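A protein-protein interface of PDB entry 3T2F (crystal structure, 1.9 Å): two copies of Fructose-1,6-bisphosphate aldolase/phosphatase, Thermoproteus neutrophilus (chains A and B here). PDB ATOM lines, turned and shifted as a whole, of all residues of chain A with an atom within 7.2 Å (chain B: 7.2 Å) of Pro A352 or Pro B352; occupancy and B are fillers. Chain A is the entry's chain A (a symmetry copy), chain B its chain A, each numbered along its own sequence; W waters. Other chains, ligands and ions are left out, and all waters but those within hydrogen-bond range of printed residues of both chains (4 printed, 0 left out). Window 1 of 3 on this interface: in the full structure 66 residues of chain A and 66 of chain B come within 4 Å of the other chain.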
ATOM      1  N   GLY A 195     -25.668  20.669   8.664  1.00  0.00           N
ATOM      2  CA  GLY A 195     -25.071  21.586   7.666  1.00  0.00           C
ATOM      3  C   GLY A 195     -23.657  21.176   7.385  1.00  0.00           C
ATOM      4  O   GLY A 195     -23.150  21.345   6.263  1.00  0.00           O
ATOM      5  N   THR A 196     -22.982  20.510   8.342  1.00  0.00           N
ATOM      6  CA  THR A 196     -21.623  19.957   8.095  1.00  0.00           C
ATOM      7  C   THR A 196     -21.754  18.495   7.562  1.00  0.00           C
ATOM      8  O   THR A 196     -21.737  17.451   8.332  1.00  0.00           O
ATOM      9  CB  THR A 196     -20.766  20.017   9.385  1.00  0.00           C
ATOM     10  OG1 THR A 196     -20.780  21.341   9.850  1.00  0.00           O
ATOM     11  CG2 THR A 196     -19.355  19.421   9.144  1.00  0.00           C
ATOM     12  N   HIS A 262     -21.209  17.127  -2.109  1.00  0.00           N
ATOM     13  CA  HIS A 262     -19.828  16.681  -2.219  1.00  0.00           C
ATOM     14  C   HIS A 262     -19.704  15.344  -2.881  1.00  0.00           C
ATOM     15  O   HIS A 262     -20.444  14.410  -2.579  1.00  0.00           O
ATOM     16  CB  HIS A 262     -19.199  16.513  -0.833  1.00  0.00           C
ATOM     17  CG  HIS A 262     -19.123  17.770  -0.032  1.00  0.00           C
ATOM     18  ND1 HIS A 262     -19.369  19.026  -0.563  1.00  0.00           N
ATOM     19  CD2 HIS A 262     -18.720  17.979   1.243  1.00  0.00           C
ATOM     20  CE1 HIS A 262     -19.221  19.943   0.382  1.00  0.00           C
ATOM     21  NE2 HIS A 262     -18.843  19.330   1.486  1.00  0.00           N
ATOM     22  N   SER A 268     -13.940  14.402  -4.944  1.00  0.00           N
ATOM     23  CA  SER A 268     -13.215  15.595  -4.459  1.00  0.00           C
ATOM     24  C   SER A 268     -13.778  16.959  -4.919  1.00  0.00           C
ATOM     25  O   SER A 268     -13.089  17.982  -4.841  1.00  0.00           O
ATOM     26  CB  SER A 268     -11.772  15.528  -4.965  1.00  0.00           C
ATOM     27  OG  SER A 268     -11.072  14.444  -4.373  1.00  0.00           O
ATOM     28  N   GLN A 347     -11.392  25.588  -4.368  1.00  0.00           N
ATOM     29  CA  GLN A 347     -12.553  25.625  -3.486  1.00  0.00           C
ATOM     30  C   GLN A 347     -13.420  26.837  -3.858  1.00  0.00           C
ATOM     31  O   GLN A 347     -12.890  27.867  -4.173  1.00  0.00           O
ATOM     32  CB  GLN A 347     -12.141  25.881  -2.003  1.00  0.00           C
ATOM     33  CG  GLN A 347     -11.697  24.544  -1.362  1.00  0.00           C
ATOM     34  CD  GLN A 347     -11.344  24.738   0.089  1.00  0.00           C
ATOM     35  OE1 GLN A 347     -10.173  24.930   0.365  1.00  0.00           O
ATOM     36  NE2 GLN A 347     -12.332  24.797   0.981  1.00  0.00           N
ATOM     37  N   PRO A 348     -14.741  26.741  -3.685  1.00  0.00           N
ATOM     38  CA  PRO A 348     -15.449  25.567  -3.102  1.00  0.00           C
ATOM     39  C   PRO A 348     -15.912  24.536  -4.145  1.00  0.00           C
ATOM     40  O   PRO A 348     -16.632  23.571  -3.758  1.00  0.00           O
ATOM     41  CB  PRO A 348     -16.665  26.206  -2.398  1.00  0.00           C
ATOM     42  CG  PRO A 348     -16.968  27.444  -3.330  1.00  0.00           C
ATOM     43  CD  PRO A 348     -15.604  27.967  -3.746  1.00  0.00           C
ATOM     44  N   HIS A 349     -15.504  24.659  -5.405  1.00  0.00           N
ATOM     45  CA  HIS A 349     -15.847  23.617  -6.347  1.00  0.00           C
ATOM     46  C   HIS A 349     -14.976  22.357  -5.995  1.00  0.00           C
ATOM     47  O   HIS A 349     -15.462  21.232  -5.983  1.00  0.00           O
ATOM     48  CB  HIS A 349     -15.558  24.047  -7.773  1.00  0.00           C
ATOM     49  CG  HIS A 349     -15.755  22.918  -8.782  1.00  0.00           C
ATOM     50  ND1 HIS A 349     -16.839  22.067  -8.744  1.00  0.00           N
ATOM     51  CD2 HIS A 349     -14.985  22.492  -9.828  1.00  0.00           C
ATOM     52  CE1 HIS A 349     -16.751  21.196  -9.748  1.00  0.00           C
ATOM     53  NE2 HIS A 349     -15.646  21.439 -10.412  1.00  0.00           N
ATOM     54  N   ARG A 350     -13.691  22.543  -5.769  1.00  0.00           N
ATOM     55  CA  ARG A 350     -12.881  21.415  -5.188  1.00  0.00           C
ATOM     56  C   ARG A 350     -13.176  21.439  -3.681  1.00  0.00           C
ATOM     57  O   ARG A 350     -13.403  22.515  -3.071  1.00  0.00           O
ATOM     58  CB  ARG A 350     -11.390  21.761  -5.308  1.00  0.00           C
ATOM     59  CG  ARG A 350     -10.464  20.533  -5.317  1.00  0.00           C
ATOM     60  CD  ARG A 350      -9.093  20.887  -4.496  1.00  0.00           C
ATOM     61  NE  ARG A 350      -9.307  21.287  -3.084  1.00  0.00           N
ATOM     62  CZ  ARG A 350      -8.413  21.945  -2.359  1.00  0.00           C
ATOM     63  NH1 ARG A 350      -8.686  22.200  -1.126  1.00  0.00           N
ATOM     64  NH2 ARG A 350      -7.268  22.372  -2.927  1.00  0.00           N
ATOM     65  N   LEU A 351     -13.234  20.257  -3.027  1.00  0.00           N
ATOM     66  CA  LEU A 351     -13.593  20.252  -1.614  1.00  0.00           C
ATOM     67  C   LEU A 351     -12.466  20.760  -0.683  1.00  0.00           C
ATOM     68  O   LEU A 351     -11.336  20.850  -1.109  1.00  0.00           O
ATOM     69  CB  LEU A 351     -13.861  18.791  -1.245  1.00  0.00           C
ATOM     70  CG  LEU A 351     -15.160  18.287  -1.956  1.00  0.00           C
ATOM     71  CD1 LEU A 351     -15.380  16.853  -1.510  1.00  0.00           C
ATOM     72  CD2 LEU A 351     -16.391  19.206  -1.655  1.00  0.00           C
ATOM     73  N   PRO A 352     -12.783  21.000   0.588  1.00  0.00           N
ATOM     74  CA  PRO A 352     -11.867  21.405   1.646  1.00  0.00           C
ATOM     75  C   PRO A 352     -10.794  20.292   1.790  1.00  0.00           C
ATOM     76  O   PRO A 352     -11.047  19.172   1.469  1.00  0.00           O
ATOM     77  CB  PRO A 352     -12.789  21.446   2.878  1.00  0.00           C
ATOM     78  CG  PRO A 352     -14.062  21.766   2.336  1.00  0.00           C
ATOM     79  CD  PRO A 352     -14.172  21.062   1.063  1.00  0.00           C
ATOM     80  N   PRO A 353      -9.561  20.644   2.134  1.00  0.00           N
ATOM     81  CA  PRO A 353      -8.467  19.647   2.005  1.00  0.00           C
ATOM     82  C   PRO A 353      -8.695  18.396   2.965  1.00  0.00           C
ATOM     83  O   PRO A 353      -8.379  17.290   2.625  1.00  0.00           O
ATOM     84  CB  PRO A 353      -7.210  20.441   2.396  1.00  0.00           C
ATOM     85  CG  PRO A 353      -7.723  21.659   3.225  1.00  0.00           C
ATOM     86  CD  PRO A 353      -9.156  21.943   2.668  1.00  0.00           C
ATOM     87  N   GLU A 354      -9.400  18.583   4.063  1.00  0.00           N
ATOM     88  CA  GLU A 354      -9.641  17.471   4.968  1.00  0.00           C
ATOM     89  C   GLU A 354     -10.742  16.564   4.444  1.00  0.00           C
ATOM     90  O   GLU A 354     -10.812  15.459   4.908  1.00  0.00           O
ATOM     91  CB  GLU A 354     -10.088  18.053   6.294  1.00  0.00           C
ATOM     92  CG  GLU A 354      -9.812  19.600   6.258  1.00  0.00           C
ATOM     93  CD  GLU A 354     -11.011  20.458   5.790  1.00  0.00           C
ATOM     94  OE1 GLU A 354     -10.731  21.609   5.383  1.00  0.00           O
ATOM     95  OE2 GLU A 354     -12.221  20.036   5.881  1.00  0.00           O
ATOM     96  N   GLU A 355     -11.594  17.039   3.504  1.00  0.00           N
ATOM     97  CA  GLU A 355     -12.718  16.287   2.948  1.00  0.00           C
ATOM     98  C   GLU A 355     -12.421  15.648   1.641  1.00  0.00           C
ATOM     99  O   GLU A 355     -13.331  15.057   1.047  1.00  0.00           O
ATOM    100  CB  GLU A 355     -14.008  17.153   2.771  1.00  0.00           C
ATOM    101  CG  GLU A 355     -14.214  18.128   3.986  1.00  0.00           C
ATOM    102  CD  GLU A 355     -15.673  18.679   4.205  1.00  0.00           C
ATOM    103  OE1 GLU A 355     -15.842  19.853   4.708  1.00  0.00           O
ATOM    104  OE2 GLU A 355     -16.654  17.916   3.947  1.00  0.00           O
ATOM    105  N   MET A 356     -11.168  15.730   1.188  1.00  0.00           N
ATOM    106  CA  MET A 356     -10.831  15.294  -0.170  1.00  0.00           C
ATOM    107  C   MET A 356     -10.731  13.792  -0.093  1.00  0.00           C
ATOM    108  O   MET A 356     -10.129  13.311   0.856  1.00  0.00           O
ATOM    109  CB  MET A 356      -9.448  15.828  -0.575  1.00  0.00           C
ATOM    110  CG  MET A 356      -9.312  17.299  -0.544  1.00  0.00           C
ATOM    111  SD  MET A 356      -9.935  17.807  -2.120  1.00  0.00           S
ATOM    112  CE  MET A 356      -8.533  17.288  -3.184  1.00  0.00           C
ATOM    113  N   GLU A 357     -11.320  13.064  -1.057  1.00  0.00           N
ATOM    114  CA  GLU A 357     -10.977  11.630  -1.284  1.00  0.00           C
ATOM    115  C   GLU A 357      -9.517  11.440  -1.859  1.00  0.00           C
ATOM    116  O   GLU A 357      -8.748  10.570  -1.355  1.00  0.00           O
ATOM    117  CB  GLU A 357     -12.082  10.900  -2.109  1.00  0.00           C
ATOM    118  CG  GLU A 357     -12.044   9.343  -2.094  1.00  0.00           C
ATOM    119  CD  GLU A 357     -12.397   8.694  -3.487  1.00  0.00           C
ATOM    120  OE1 GLU A 357     -13.566   8.801  -3.972  1.00  0.00           O
ATOM    121  OE2 GLU A 357     -11.488   8.069  -4.108  1.00  0.00           O
ATOM    122  N   GLY B 195      -5.643  26.263  -4.572  1.00  0.00           N
ATOM    123  CA  GLY B 195      -7.026  25.734  -4.600  1.00  0.00           C
ATOM    124  C   GLY B 195      -7.592  25.725  -3.212  1.00  0.00           C
ATOM    125  O   GLY B 195      -8.805  25.904  -3.011  1.00  0.00           O
ATOM    126  N   THR B 196      -6.737  25.636  -2.173  1.00  0.00           N
ATOM    127  CA  THR B 196      -7.207  25.750  -0.766  1.00  0.00           C
ATOM    128  C   THR B 196      -7.147  27.247  -0.326  1.00  0.00           C
ATOM    129  O   THR B 196      -6.121  27.776   0.265  1.00  0.00           O
ATOM    130  CB  THR B 196      -6.359  24.849   0.167  1.00  0.00           C
ATOM    131  OG1 THR B 196      -6.386  23.545  -0.352  1.00  0.00           O
ATOM    132  CG2 THR B 196      -6.825  24.978   1.640  1.00  0.00           C
ATOM    133  N   HIS B 262     -15.431  32.434  -0.748  1.00  0.00           N
ATOM    134  CA  HIS B 262     -15.822  32.392   0.652  1.00  0.00           C
ATOM    135  C   HIS B 262     -16.000  33.755   1.244  1.00  0.00           C
ATOM    136  O   HIS B 262     -15.181  34.650   1.043  1.00  0.00           O
ATOM    137  CB  HIS B 262     -14.739  31.715   1.499  1.00  0.00           C
ATOM    138  CG  HIS B 262     -14.476  30.290   1.141  1.00  0.00           C
ATOM    139  ND1 HIS B 262     -15.288  29.557   0.291  1.00  0.00           N
ATOM    140  CD2 HIS B 262     -13.545  29.423   1.605  1.00  0.00           C
ATOM    141  CE1 HIS B 262     -14.806  28.328   0.169  1.00  0.00           C
ATOM    142  NE2 HIS B 262     -13.743  28.230   0.943  1.00  0.00           N
ATOM    143  N   SER B 268     -19.361  33.511   6.441  1.00  0.00           N
ATOM    144  CA  SER B 268     -19.563  32.061   6.637  1.00  0.00           C
ATOM    145  C   SER B 268     -20.248  31.312   5.471  1.00  0.00           C
ATOM    146  O   SER B 268     -20.742  30.193   5.647  1.00  0.00           O
ATOM    147  CB  SER B 268     -20.452  31.854   7.866  1.00  0.00           C
ATOM    148  OG  SER B 268     -19.789  32.265   9.052  1.00  0.00           O
ATOM    149  N   GLN B 347     -23.416  23.070   3.898  1.00  0.00           N
ATOM    150  CA  GLN B 347     -22.275  23.042   2.991  1.00  0.00           C
ATOM    151  C   GLN B 347     -22.733  22.484   1.636  1.00  0.00           C
ATOM    152  O   GLN B 347     -23.527  21.584   1.605  1.00  0.00           O
ATOM    153  CB  GLN B 347     -21.179  22.042   3.474  1.00  0.00           C
ATOM    154  CG  GLN B 347     -20.306  22.729   4.552  1.00  0.00           C
ATOM    155  CD  GLN B 347     -19.199  21.814   5.005  1.00  0.00           C
ATOM    156  OE1 GLN B 347     -19.395  21.141   6.002  1.00  0.00           O
ATOM    157  NE2 GLN B 347     -18.111  21.707   4.243  1.00  0.00           N
ATOM    158  N   PRO B 348     -22.124  22.931   0.534  1.00  0.00           N
ATOM    159  CA  PRO B 348     -20.987  23.893   0.510  1.00  0.00           C
ATOM    160  C   PRO B 348     -21.417  25.364   0.389  1.00  0.00           C
ATOM    161  O   PRO B 348     -20.520  26.242   0.233  1.00  0.00           O
ATOM    162  CB  PRO B 348     -20.187  23.459  -0.737  1.00  0.00           C
ATOM    163  CG  PRO B 348     -21.330  22.935  -1.691  1.00  0.00           C
ATOM    164  CD  PRO B 348     -22.311  22.223  -0.777  1.00  0.00           C
ATOM    165  N   HIS B 349     -22.705  25.676   0.500  1.00  0.00           N
ATOM    166  CA  HIS B 349     -23.080  27.072   0.506  1.00  0.00           C
ATOM    167  C   HIS B 349     -22.626  27.678   1.882  1.00  0.00           C
ATOM    168  O   HIS B 349     -22.082  28.775   1.946  1.00  0.00           O
ATOM    169  CB  HIS B 349     -24.580  27.240   0.352  1.00  0.00           C
ATOM    170  CG  HIS B 349     -25.032  28.690   0.514  1.00  0.00           C
ATOM    171  ND1 HIS B 349     -24.366  29.747  -0.068  1.00  0.00           N
ATOM    172  CD2 HIS B 349     -26.063  29.244   1.220  1.00  0.00           C
ATOM    173  CE1 HIS B 349     -24.992  30.883   0.234  1.00  0.00           C
ATOM    174  NE2 HIS B 349     -26.016  30.599   1.004  1.00  0.00           N
ATOM    175  N   ARG B 350     -22.900  26.994   2.975  1.00  0.00           N
ATOM    176  CA  ARG B 350     -22.267  27.409   4.276  1.00  0.00           C
ATOM    177  C   ARG B 350     -20.845  26.829   4.239  1.00  0.00           C
ATOM    178  O   ARG B 350     -20.593  25.741   3.662  1.00  0.00           O
ATOM    179  CB  ARG B 350     -22.968  26.674   5.427  1.00  0.00           C
ATOM    180  CG  ARG B 350     -22.861  27.392   6.783  1.00  0.00           C
ATOM    181  CD  ARG B 350     -22.692  26.278   7.970  1.00  0.00           C
ATOM    182  NE  ARG B 350     -21.507  25.399   7.826  1.00  0.00           N
ATOM    183  CZ  ARG B 350     -21.372  24.234   8.442  1.00  0.00           C
ATOM    184  NH1 ARG B 350     -20.278  23.573   8.281  1.00  0.00           N
ATOM    185  NH2 ARG B 350     -22.385  23.742   9.181  1.00  0.00           N
ATOM    186  N   LEU B 351     -19.851  27.550   4.805  1.00  0.00           N
ATOM    187  CA  LEU B 351     -18.483  27.057   4.709  1.00  0.00           C
ATOM    188  C   LEU B 351     -18.190  25.848   5.630  1.00  0.00           C
ATOM    189  O   LEU B 351     -18.960  25.581   6.526  1.00  0.00           O
ATOM    190  CB  LEU B 351     -17.580  28.204   5.167  1.00  0.00           C
ATOM    191  CG  LEU B 351     -17.624  29.371   4.127  1.00  0.00           C
ATOM    192  CD1 LEU B 351     -16.678  30.447   4.628  1.00  0.00           C
ATOM    193  CD2 LEU B 351     -17.271  28.885   2.681  1.00  0.00           C
ATOM    194  N   PRO B 352     -17.043  25.198   5.442  1.00  0.00           N
ATOM    195  CA  PRO B 352     -16.535  24.091   6.241  1.00  0.00           C
ATOM    196  C   PRO B 352     -16.379  24.597   7.701  1.00  0.00           C
ATOM    197  O   PRO B 352     -16.207  25.758   7.916  1.00  0.00           O
ATOM    198  CB  PRO B 352     -15.162  23.827   5.597  1.00  0.00           C
ATOM    199  CG  PRO B 352     -15.341  24.223   4.245  1.00  0.00           C
ATOM    200  CD  PRO B 352     -16.197  25.405   4.258  1.00  0.00           C
ATOM    201  N   PRO B 353     -16.587  23.740   8.693  1.00  0.00           N
ATOM    202  CA  PRO B 353     -16.718  24.262  10.077  1.00  0.00           C
ATOM    203  C   PRO B 353     -15.376  24.963  10.571  1.00  0.00           C
ATOM    204  O   PRO B 353     -15.407  25.929  11.282  1.00  0.00           O
ATOM    205  CB  PRO B 353     -17.042  23.007  10.905  1.00  0.00           C
ATOM    206  CG  PRO B 353     -16.550  21.800  10.046  1.00  0.00           C
ATOM    207  CD  PRO B 353     -16.679  22.287   8.566  1.00  0.00           C
ATOM    208  N   GLU B 354     -14.240  24.563  10.036  1.00  0.00           N
ATOM    209  CA  GLU B 354     -12.988  25.176  10.448  1.00  0.00           C
ATOM    210  C   GLU B 354     -12.795  26.532   9.788  1.00  0.00           C
ATOM    211  O   GLU B 354     -11.991  27.275  10.282  1.00  0.00           O
ATOM    212  CB  GLU B 354     -11.864  24.261  10.005  1.00  0.00           C
ATOM    213  CG  GLU B 354     -12.504  22.893   9.567  1.00  0.00           C
ATOM    214  CD  GLU B 354     -12.821  22.783   8.057  1.00  0.00           C
ATOM    215  OE1 GLU B 354     -13.657  21.906   7.739  1.00  0.00           O
ATOM    216  OE2 GLU B 354     -12.211  23.501   7.184  1.00  0.00           O
ATOM    217  N   GLU B 355     -13.513  26.832   8.681  1.00  0.00           N
ATOM    218  CA  GLU B 355     -13.394  28.079   7.926  1.00  0.00           C
ATOM    219  C   GLU B 355     -14.432  29.084   8.266  1.00  0.00           C
ATOM    220  O   GLU B 355     -14.468  30.142   7.625  1.00  0.00           O
ATOM    221  CB  GLU B 355     -13.427  27.865   6.378  1.00  0.00           C
ATOM    222  CG  GLU B 355     -12.611  26.590   5.958  1.00  0.00           C
ATOM    223  CD  GLU B 355     -12.133  26.523   4.458  1.00  0.00           C
ATOM    224  OE1 GLU B 355     -12.028  25.380   3.874  1.00  0.00           O
ATOM    225  OE2 GLU B 355     -11.791  27.601   3.883  1.00  0.00           O
ATOM    226  N   MET B 356     -15.263  28.793   9.269  1.00  0.00           N
ATOM    227  CA  MET B 356     -16.429  29.638   9.547  1.00  0.00           C
ATOM    228  C   MET B 356     -15.889  30.824  10.304  1.00  0.00           C
ATOM    229  O   MET B 356     -15.080  30.609  11.195  1.00  0.00           O
ATOM    230  CB  MET B 356     -17.410  28.906  10.477  1.00  0.00           C
ATOM    231  CG  MET B 356     -17.919  27.619   9.959  1.00  0.00           C
ATOM    232  SD  MET B 356     -19.285  28.092   8.940  1.00  0.00           S
ATOM    233  CE  MET B 356     -20.503  28.521  10.244  1.00  0.00           C
ATOM    234  N   GLU B 357     -16.310  32.051   9.952  1.00  0.00           N
ATOM    235  CA  GLU B 357     -16.140  33.232  10.846  1.00  0.00           C
ATOM    236  C   GLU B 357     -17.054  33.153  12.134  1.00  0.00           C
ATOM    237  O   GLU B 357     -16.563  33.401  13.274  1.00  0.00           O
ATOM    238  CB  GLU B 357     -16.272  34.572  10.059  1.00  0.00           C
ATOM    239  CG  GLU B 357     -15.749  35.852  10.775  1.00  0.00           C
ATOM    240  CD  GLU B 357     -16.652  37.121  10.530  1.00  0.00           C
ATOM    241  OE1 GLU B 357     -16.743  37.636   9.372  1.00  0.00           O
ATOM    242  OE2 GLU B 357     -17.284  37.610  11.511  1.00  0.00           O
HETATM  243  O   HOH W   1      -9.751  26.909   2.355  1.00  0.00           O
HETATM  244  O   HOH W   2     -15.167  25.350   0.552  1.00  0.00           O
HETATM  245  O   HOH W   3     -17.768  22.383   1.423  1.00  0.00           O
HETATM  246  O   HOH W   4     -18.430  18.478   5.820  1.00  0.00           O
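Gly A195 touches Arg B350, and with the chains exchanged Arg A350 touches Gly B195.
Thr A196 touches Gln B347, and with the chains exchanged Gln A347 touches Thr B196.
Thr A196 touches Arg B350, and with the chains exchanged Arg A350 touches Thr B196.
Glu A354 touches its own counterpart, Glu B354.
Of the 18 pairs that touch across the chains among the printed residues, 18 have their exchanged pair printed and touching as well.
Of the 15 printed residues of chain A, 10 touch a printed residue of chain B.
Of the 15 printed residues of chain B, 10 touch a printed residue of chain A.
Printed residues of chain B that touch a printed residue of chain A: Gly B195, Thr B196, His B262, Gln B347, Pro B348, Arg B350, Pro B352, Pro B353, Glu B354 and Glu B355.
Hydrophobic or aromatic side chains of chain B that line the printed part of chain A: His B262, Pro B348, Pro B352 and Pro B353.
The backbone carbonyl oxygen (O) of Gly B195 lies within hydrogen-bond range of the backbone NH (N) of Gln A347, at 2.9 Å.
The guanidinium group of Arg A350 lies within hydrogen-bond range of the side-chain hydroxyl of Thr B196 (2.8 Å).
O of Gly A195 lies within hydrogen-bond range of N of Gln B347 (2.9 Å).
The side-chain carboxylate (OE1) of Glu A355 lies within hydrogen-bond range of the side-chain amide nitrogen (NE2) of Gln B347 (3.0 Å).
The side-chain hydroxyl (OG1) of Thr A196 sits at hydrogen-bond distance from the guanidinium group (NH1) of Arg B350 (2.8 Å).
OE1 of Glu B355 lies within hydrogen-bond range of NE2 of Gln A347 (3.0 Å).
The side-chain carboxylate (OE2) of Glu A354 sits close to the side-chain carboxylate (OE1) of Glu B354, 3.0 Å away.
Among the printed residues, merely in contact across the chains: Gly A195 with Arg B350 (3.4 Å), Thr A196 with Gln B347 (3.3 Å), Thr A196 with Pro B353 (3.8 Å), His A262 with Gln B347 (3.7 Å), His A262 with Pro B348 (3.8 Å), Gln A347 with Thr B196 (3.3 Å), Gln A347 with His B262 (3.7 Å), Pro A348 with His B262 (3.8 Å), Arg A350 with Gly B195 (3.4 Å), Pro A352 with Pro B352 (3.4 Å) and Pro A353 with Thr B196 (3.8 Å).
Printed residues of chain B within 4 Å of Thr A196: Gln B347 (3.3 Å), Arg B350 (2.8 Å) and Pro B353 (3.8 Å).
Of chain B, only Pro B352 comes within 4 Å of Pro A352.
Printed residues of chain A within 4 Å of Gly B195: Gln A347 and Arg A350.
Printed residues of chain A within 4 Å of Thr B196: Gln A347 (3.3 Å), Arg A350 (2.8 Å) and Pro A353 (3.8 Å).
Of the printed residues of chain A, Arg B350 touches Gly A195 and Thr A196.
Of chain A, only Pro A352 (3.4 Å) comes within 4 Å of Pro B352.
Met B356 touches none of the printed residues of chain A.
Glu B357 touches none of the printed residues of chain A.
OE1 of Gln B347 sits at hydrogen-bond distance from NH1 of Arg B350, 3.4 Å away.
SD of Met B356 lies within hydrogen-bond range of NE of Arg B350 (3.7 Å).
OE1 of Gln A347 sits at hydrogen-bond distance from NH1 of Arg A350 (3.4 Å).
The guanidinium group (NE) of Arg A350 is in hydrogen-bond range of the side-chain sulfur (SD) of Met A356 (3.7 Å).
Water W1 lies within hydrogen-bond range of OE2 of Glu B355 (2.6 Å) and OE1 of Gln A347 (2.8 Å).
Water W4 lies within hydrogen-bond range of the side-chain carboxylate (OE2) of Glu A355 (2.6 Å) and the side-chain amide oxygen (OE1) of Gln B347 (2.8 Å).
Water W2 lies within hydrogen-bond range of the side-chain amide nitrogen (NE2) of Gln A347 and a ring nitrogen (NE2) of His B262.
Water W3 lies within hydrogen-bond range of the side-chain amide nitrogen (NE2) of Gln B347 (2.9 Å) and a ring nitrogen (NE2) of His A262 (3.2 Å).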
